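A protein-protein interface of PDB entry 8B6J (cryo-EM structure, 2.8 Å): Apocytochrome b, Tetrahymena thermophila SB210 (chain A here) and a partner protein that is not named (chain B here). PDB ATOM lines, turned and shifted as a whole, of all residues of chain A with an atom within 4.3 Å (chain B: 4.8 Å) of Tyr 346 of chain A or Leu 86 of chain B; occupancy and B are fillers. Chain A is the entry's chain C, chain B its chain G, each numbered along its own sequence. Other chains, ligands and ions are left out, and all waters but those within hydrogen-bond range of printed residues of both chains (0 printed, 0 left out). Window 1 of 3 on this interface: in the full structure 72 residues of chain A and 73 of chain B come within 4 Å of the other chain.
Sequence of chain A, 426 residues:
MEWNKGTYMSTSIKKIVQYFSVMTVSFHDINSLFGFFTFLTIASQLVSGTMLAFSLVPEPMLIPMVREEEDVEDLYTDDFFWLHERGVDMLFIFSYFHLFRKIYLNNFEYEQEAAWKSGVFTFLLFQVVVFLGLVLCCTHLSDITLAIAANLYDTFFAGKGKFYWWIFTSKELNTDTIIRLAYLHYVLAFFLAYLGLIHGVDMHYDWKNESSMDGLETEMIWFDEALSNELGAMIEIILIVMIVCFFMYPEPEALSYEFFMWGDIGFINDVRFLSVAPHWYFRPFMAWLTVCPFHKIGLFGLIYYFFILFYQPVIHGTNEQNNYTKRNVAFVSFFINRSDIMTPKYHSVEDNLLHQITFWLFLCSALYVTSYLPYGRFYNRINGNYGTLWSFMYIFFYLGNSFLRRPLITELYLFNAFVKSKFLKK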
ATOM      1  N   PRO A 344       7.610   2.050   3.221  1.00  0.00           N
ATOM      2  CA  PRO A 344       8.358   2.665   4.321  1.00  0.00           C
ATOM      3  C   PRO A 344       8.294   4.183   4.264  1.00  0.00           C
ATOM      4  O   PRO A 344       8.100   4.781   3.205  1.00  0.00           O
ATOM      5  CB  PRO A 344       9.787   2.157   4.108  1.00  0.00           C
ATOM      6  CG  PRO A 344       9.860   1.833   2.665  1.00  0.00           C
ATOM      7  CD  PRO A 344       8.499   1.337   2.290  1.00  0.00           C
ATOM      8  N   LYS A 345       8.462   4.804   5.429  1.00  0.00           N
ATOM      9  CA  LYS A 345       8.307   6.246   5.580  1.00  0.00           C
ATOM     10  C   LYS A 345       9.620   6.991   5.763  1.00  0.00           C
ATOM     11  O   LYS A 345       9.829   8.018   5.115  1.00  0.00           O
ATOM     12  CB  LYS A 345       7.398   6.553   6.776  1.00  0.00           C
ATOM     13  CG  LYS A 345       6.969   8.008   6.864  1.00  0.00           C
ATOM     14  CD  LYS A 345       5.986   8.237   7.998  1.00  0.00           C
ATOM     15  CE  LYS A 345       6.666   8.148   9.351  1.00  0.00           C
ATOM     16  NZ  LYS A 345       5.718   8.399  10.468  1.00  0.00           N
ATOM     17  N   TYR A 346      10.516   6.505   6.622  1.00  0.00           N
ATOM     18  CA  TYR A 346      11.707   7.261   7.012  1.00  0.00           C
ATOM     19  C   TYR A 346      12.772   7.219   5.913  1.00  0.00           C
ATOM     20  O   TYR A 346      13.901   6.770   6.106  1.00  0.00           O
ATOM     21  CB  TYR A 346      12.256   6.723   8.327  1.00  0.00           C
ATOM     22  CG  TYR A 346      11.305   6.857   9.494  1.00  0.00           C
ATOM     23  CD1 TYR A 346      10.547   8.005   9.672  1.00  0.00           C
ATOM     24  CD2 TYR A 346      11.160   5.831  10.417  1.00  0.00           C
ATOM     25  CE1 TYR A 346       9.680   8.130  10.735  1.00  0.00           C
ATOM     26  CE2 TYR A 346      10.294   5.947  11.483  1.00  0.00           C
ATOM     27  CZ  TYR A 346       9.555   7.098  11.637  1.00  0.00           C
ATOM     28  OH  TYR A 346       8.690   7.221  12.696  1.00  0.00           O
ATOM     29  N   HIS A 347      12.391   7.717   4.742  1.00  0.00           N
ATOM     30  CA  HIS A 347      13.292   7.778   3.592  1.00  0.00           C
ATOM     31  C   HIS A 347      13.955   9.152   3.504  1.00  0.00           C
ATOM     32  O   HIS A 347      13.853   9.866   2.507  1.00  0.00           O
ATOM     33  CB  HIS A 347      12.537   7.436   2.309  1.00  0.00           C
ATOM     34  CG  HIS A 347      11.413   8.375   1.998  1.00  0.00           C
ATOM     35  ND1 HIS A 347      10.215   8.355   2.678  1.00  0.00           N
ATOM     36  CD2 HIS A 347      11.302   9.355   1.070  1.00  0.00           C
ATOM     37  CE1 HIS A 347       9.418   9.288   2.190  1.00  0.00           C
ATOM     38  NE2 HIS A 347      10.053   9.908   1.212  1.00  0.00           N
ATOM     39  N   SER A 348      14.656   9.516   4.574  1.00  0.00           N
ATOM     40  CA  SER A 348      15.383  10.776   4.598  1.00  0.00           C
ATOM     41  C   SER A 348      16.512  10.741   3.570  1.00  0.00           C
ATOM     42  O   SER A 348      16.761   9.729   2.910  1.00  0.00           O
ATOM     43  CB  SER A 348      15.918  11.053   6.000  1.00  0.00           C
ATOM     44  OG  SER A 348      16.774  10.013   6.434  1.00  0.00           O
ATOM     45  N   ASN A 352      20.385   9.542   5.622  1.00  0.00           N
ATOM     46  CA  ASN A 352      20.185   8.184   5.132  1.00  0.00           C
ATOM     47  C   ASN A 352      21.402   7.779   4.309  1.00  0.00           C
ATOM     48  O   ASN A 352      21.674   8.365   3.257  1.00  0.00           O
ATOM     49  CB  ASN A 352      18.904   8.095   4.307  1.00  0.00           C
ATOM     50  CG  ASN A 352      18.531   6.670   3.967  1.00  0.00           C
ATOM     51  OD1 ASN A 352      18.950   6.134   2.942  1.00  0.00           O
ATOM     52  ND2 ASN A 352      17.739   6.045   4.828  1.00  0.00           N
ATOM     53  N   THR A 410      15.129   0.174   6.219  1.00  0.00           N
ATOM     54  CA  THR A 410      15.413   1.432   6.903  1.00  0.00           C
ATOM     55  C   THR A 410      14.429   1.672   8.039  1.00  0.00           C
ATOM     56  O   THR A 410      14.822   2.050   9.148  1.00  0.00           O
ATOM     57  CB  THR A 410      15.371   2.593   5.909  1.00  0.00           C
ATOM     58  OG1 THR A 410      16.431   2.453   4.955  1.00  0.00           O
ATOM     59  CG2 THR A 410      15.515   3.921   6.634  1.00  0.00           C
ATOM     60  N   GLU A 411      13.141   1.456   7.780  1.00  0.00           N
ATOM     61  CA  GLU A 411      12.124   1.657   8.803  1.00  0.00           C
ATOM     62  C   GLU A 411      11.918   0.427   9.673  1.00  0.00           C
ATOM     63  O   GLU A 411      11.546   0.563  10.843  1.00  0.00           O
ATOM     64  CB  GLU A 411      10.795   2.057   8.157  1.00  0.00           C
ATOM     65  CG  GLU A 411       9.694   2.367   9.159  1.00  0.00           C
ATOM     66  CD  GLU A 411       8.604   3.247   8.579  1.00  0.00           C
ATOM     67  OE1 GLU A 411       8.909   4.071   7.693  1.00  0.00           O
ATOM     68  OE2 GLU A 411       7.438   3.117   9.010  1.00  0.00           O
ATOM     69  N   LEU A 414      14.504   0.586  12.377  1.00  0.00           N
ATOM     70  CA  LEU A 414      14.158   1.679  13.277  1.00  0.00           C
ATOM     71  C   LEU A 414      13.024   1.279  14.208  1.00  0.00           C
ATOM     72  O   LEU A 414      13.045   1.607  15.397  1.00  0.00           O
ATOM     73  CB  LEU A 414      13.782   2.922  12.473  1.00  0.00           C
ATOM     74  CG  LEU A 414      14.941   3.675  11.818  1.00  0.00           C
ATOM     75  CD1 LEU A 414      14.415   4.777  10.915  1.00  0.00           C
ATOM     76  CD2 LEU A 414      15.875   4.250  12.871  1.00  0.00           C
ATOM     77  N   PHE A 418      12.942   1.066  18.213  1.00  0.00           N
ATOM     78  CA  PHE A 418      11.906   1.741  18.987  1.00  0.00           C
ATOM     79  C   PHE A 418      11.270   0.786  19.984  1.00  0.00           C
ATOM     80  O   PHE A 418      11.084   1.124  21.159  1.00  0.00           O
ATOM     81  CB  PHE A 418      10.829   2.312  18.063  1.00  0.00           C
ATOM     82  CG  PHE A 418      11.332   3.319  17.067  1.00  0.00           C
ATOM     83  CD1 PHE A 418      12.584   3.896  17.192  1.00  0.00           C
ATOM     84  CD2 PHE A 418      10.533   3.694  16.000  1.00  0.00           C
ATOM     85  CE1 PHE A 418      13.027   4.821  16.270  1.00  0.00           C
ATOM     86  CE2 PHE A 418      10.971   4.616  15.078  1.00  0.00           C
ATOM     87  CZ  PHE A 418      12.218   5.180  15.212  1.00  0.00           C
ATOM     88  N   ARG B  71      22.652   8.728  12.058  1.00  0.00           N
ATOM     89  CA  ARG B  71      21.592   9.720  12.197  1.00  0.00           C
ATOM     90  C   ARG B  71      21.752  10.512  13.484  1.00  0.00           C
ATOM     91  O   ARG B  71      21.572  11.735  13.495  1.00  0.00           O
ATOM     92  CB  ARG B  71      20.226   9.033  12.178  1.00  0.00           C
ATOM     93  CG  ARG B  71      19.844   8.402  10.854  1.00  0.00           C
ATOM     94  CD  ARG B  71      18.572   7.581  10.995  1.00  0.00           C
ATOM     95  NE  ARG B  71      18.043   7.157   9.704  1.00  0.00           N
ATOM     96  CZ  ARG B  71      17.215   7.874   8.959  1.00  0.00           C
ATOM     97  NH1 ARG B  71      16.795   9.070   9.341  1.00  0.00           N
ATOM     98  NH2 ARG B  71      16.794   7.381   7.798  1.00  0.00           N
ATOM     99  N   LEU B  82      16.619  12.717  17.324  1.00  0.00           N
ATOM    100  CA  LEU B  82      15.901  11.913  16.342  1.00  0.00           C
ATOM    101  C   LEU B  82      14.448  12.350  16.228  1.00  0.00           C
ATOM    102  O   LEU B  82      13.850  12.240  15.151  1.00  0.00           O
ATOM    103  CB  LEU B  82      15.986  10.431  16.708  1.00  0.00           C
ATOM    104  CG  LEU B  82      17.379   9.798  16.654  1.00  0.00           C
ATOM    105  CD1 LEU B  82      17.312   8.336  17.061  1.00  0.00           C
ATOM    106  CD2 LEU B  82      17.992   9.936  15.269  1.00  0.00           C
ATOM    107  N   GLU B  83      13.866  12.851  17.318  1.00  0.00           N
ATOM    108  CA  GLU B  83      12.495  13.344  17.262  1.00  0.00           C
ATOM    109  C   GLU B  83      12.337  14.425  16.204  1.00  0.00           C
ATOM    110  O   GLU B  83      11.265  14.555  15.605  1.00  0.00           O
ATOM    111  CB  GLU B  83      12.078  13.879  18.632  1.00  0.00           C
ATOM    112  CG  GLU B  83      10.634  14.344  18.705  1.00  0.00           C
ATOM    113  CD  GLU B  83      10.247  14.826  20.088  1.00  0.00           C
ATOM    114  OE1 GLU B  83      11.088  14.734  21.007  1.00  0.00           O
ATOM    115  OE2 GLU B  83       9.104  15.296  20.259  1.00  0.00           O
ATOM    116  N   ASP B  84      13.391  15.203  15.953  1.00  0.00           N
ATOM    117  CA  ASP B  84      13.328  16.268  14.961  1.00  0.00           C
ATOM    118  C   ASP B  84      13.227  15.746  13.535  1.00  0.00           C
ATOM    119  O   ASP B  84      12.959  16.539  12.626  1.00  0.00           O
ATOM    120  CB  ASP B  84      14.556  17.169  15.092  1.00  0.00           C
ATOM    121  CG  ASP B  84      14.531  18.004  16.355  1.00  0.00           C
ATOM    122  OD1 ASP B  84      13.499  18.656  16.614  1.00  0.00           O
ATOM    123  OD2 ASP B  84      15.537  18.002  17.094  1.00  0.00           O
ATOM    124  N   SER B  85      13.434  14.456  13.314  1.00  0.00           N
ATOM    125  CA  SER B  85      13.371  13.884  11.972  1.00  0.00           C
ATOM    126  C   SER B  85      12.409  12.714  11.866  1.00  0.00           C
ATOM    127  O   SER B  85      11.765  12.550  10.827  1.00  0.00           O
ATOM    128  CB  SER B  85      14.771  13.436  11.532  1.00  0.00           C
ATOM    129  OG  SER B  85      14.727  12.822  10.257  1.00  0.00           O
ATOM    130  N   LEU B  86      12.295  11.895  12.908  1.00  0.00           N
ATOM    131  CA  LEU B  86      11.446  10.713  12.857  1.00  0.00           C
ATOM    132  C   LEU B  86       9.995  11.023  13.206  1.00  0.00           C
ATOM    133  O   LEU B  86       9.081  10.441  12.614  1.00  0.00           O
ATOM    134  CB  LEU B  86      11.995   9.640  13.799  1.00  0.00           C
ATOM    135  CG  LEU B  86      13.482   9.328  13.614  1.00  0.00           C
ATOM    136  CD1 LEU B  86      13.920   8.207  14.537  1.00  0.00           C
ATOM    137  CD2 LEU B  86      13.786   8.975  12.167  1.00  0.00           C
ATOM    138  N   LEU B  87       9.762  11.926  14.160  1.00  0.00           N
ATOM    139  CA  LEU B  87       8.392  12.276  14.523  1.00  0.00           C
ATOM    140  C   LEU B  87       7.666  12.924  13.352  1.00  0.00           C
ATOM    141  O   LEU B  87       6.576  12.490  12.961  1.00  0.00           O
ATOM    142  CB  LEU B  87       8.396  13.206  15.735  1.00  0.00           C
ATOM    143  CG  LEU B  87       7.028  13.675  16.231  1.00  0.00           C
ATOM    144  CD1 LEU B  87       6.188  12.496  16.689  1.00  0.00           C
ATOM    145  CD2 LEU B  87       7.192  14.686  17.349  1.00  0.00           C
ATOM    146  N   PHE B  88       8.262  13.965  12.773  1.00  0.00           N
ATOM    147  CA  PHE B  88       7.712  14.650  11.611  1.00  0.00           C
ATOM    148  C   PHE B  88       8.799  14.727  10.554  1.00  0.00           C
ATOM    149  O   PHE B  88       9.837  15.357  10.775  1.00  0.00           O
ATOM    150  CB  PHE B  88       7.222  16.059  11.966  1.00  0.00           C
ATOM    151  CG  PHE B  88       6.139  16.091  13.007  1.00  0.00           C
ATOM    152  CD1 PHE B  88       5.154  15.122  13.038  1.00  0.00           C
ATOM    153  CD2 PHE B  88       6.108  17.098  13.955  1.00  0.00           C
ATOM    154  CE1 PHE B  88       4.161  15.157  13.996  1.00  0.00           C
ATOM    155  CE2 PHE B  88       5.120  17.136  14.913  1.00  0.00           C
ATOM    156  CZ  PHE B  88       4.145  16.165  14.934  1.00  0.00           C
ATOM    157  N   MET B  89       8.564  14.091   9.411  1.00  0.00           N
ATOM    158  CA  MET B  89       9.536  14.152   8.333  1.00  0.00           C
ATOM    159  C   MET B  89       9.688  15.586   7.844  1.00  0.00           C
ATOM    160  O   MET B  89       8.762  16.397   7.925  1.00  0.00           O
ATOM    161  CB  MET B  89       9.116  13.248   7.176  1.00  0.00           C
ATOM    162  CG  MET B  89       9.233  11.767   7.477  1.00  0.00           C
ATOM    163  SD  MET B  89       9.084  10.750   5.998  1.00  0.00           S
ATOM    164  CE  MET B  89      10.575  11.203   5.118  1.00  0.00           C
ATOM    165  N   ILE B 154       6.244   9.176  18.849  1.00  0.00           N
ATOM    166  CA  ILE B 154       6.042   8.685  17.486  1.00  0.00           C
ATOM    167  C   ILE B 154       4.867   7.718  17.443  1.00  0.00           C
ATOM    168  O   ILE B 154       3.996   7.808  16.568  1.00  0.00           O
ATOM    169  CB  ILE B 154       7.329   8.028  16.957  1.00  0.00           C
ATOM    170  CG1 ILE B 154       8.402   9.091  16.712  1.00  0.00           C
ATOM    171  CG2 ILE B 154       7.040   7.253  15.679  1.00  0.00           C
ATOM    172  CD1 ILE B 154       9.782   8.529  16.448  1.00  0.00           C
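Tyr 346 of chain A touches three residues of chain B. Leu 86 of chain B touches just these residues of chain A: Tyr 346 and Phe 418. Of the printed residues of chain B, Asn 352 of chain A touches Arg 71 (3.4 Å). Of the printed residues of chain A, Arg 71 of chain B touches Tyr 346, Ser 348, Asn 352 and Thr 410. Printed residues of chain B within 4 Å of Phe 418 of chain A: Leu 86 (3.5 Å). Pro 344 of chain A touches none of the printed residues of chain B. Glu 83 of chain B touches none of the printed residues of chain A. The nearest residue of chain B that does not touch Tyr 346 of chain A is Met 89 of chain B (4.5 Å). The nearest printed residue of chain A that does not touch Leu 86 of chain B is Leu 414 of chain A (4.4 Å). The nearest printed residue of chain A that does not touch Arg 71 of chain B is Leu 414 of chain A (4.5 Å).
The backbone NH (N) of Lys 345 of chain A lies within hydrogen-bond range of the side-chain carboxylate (OE1) of Glu 411 of chain A (2.4 Å). The backbone NH of Tyr 346 of chain A is in hydrogen-bond range of the side-chain carboxylate of Glu 411 of chain A (3.1 Å). O of Lys 345 of chain A is in hydrogen-bond range of ND1 of His 347 of chain A (2.5 Å).
OH of Tyr 346 of chain A lies close to O of Leu 86 of chain B. The backbone carbonyl oxygen (O) of Tyr 346 of chain A lies within hydrogen-bond range of the guanidinium group (NH2) of Arg 71 of chain B (3.4 Å). ND2 of Asn 352 of chain A lies close to NH2 of Arg 71 of chain B, 3.4 Å away. The backbone carbonyl oxygen of Lys 345 of chain A sits close to the side-chain sulfur of Met 89 of chain B, at 3.0 Å. NH2 of Arg 71 of chain B is in hydrogen-bond range of OG of Ser 348 of chain A, at 3.0 Å.
Of the 10 printed residues of chain A, 7 touch a printed residue of chain B. Along chain A the printed residues that touch a printed residue of chain B span positions 345 to 418. Hydrophobic or aromatic side chains of chain B within 4 Å of the printed part of chain A: Leu 86, Met 89 and Ile 154. Among the printed residues, 9 pairs touch across the chains.
Tyr 346 of chain A touches Ile 154 of chain B. Met 89 of chain B touches His 347 of chain A. Thr 410 of chain A touches Arg 71 of chain B (CG2 to NH2, 3.9 Å). CZ of Phe 418 of chain A touches CD1 of Leu 86 of chain B, at 3.5 Å.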
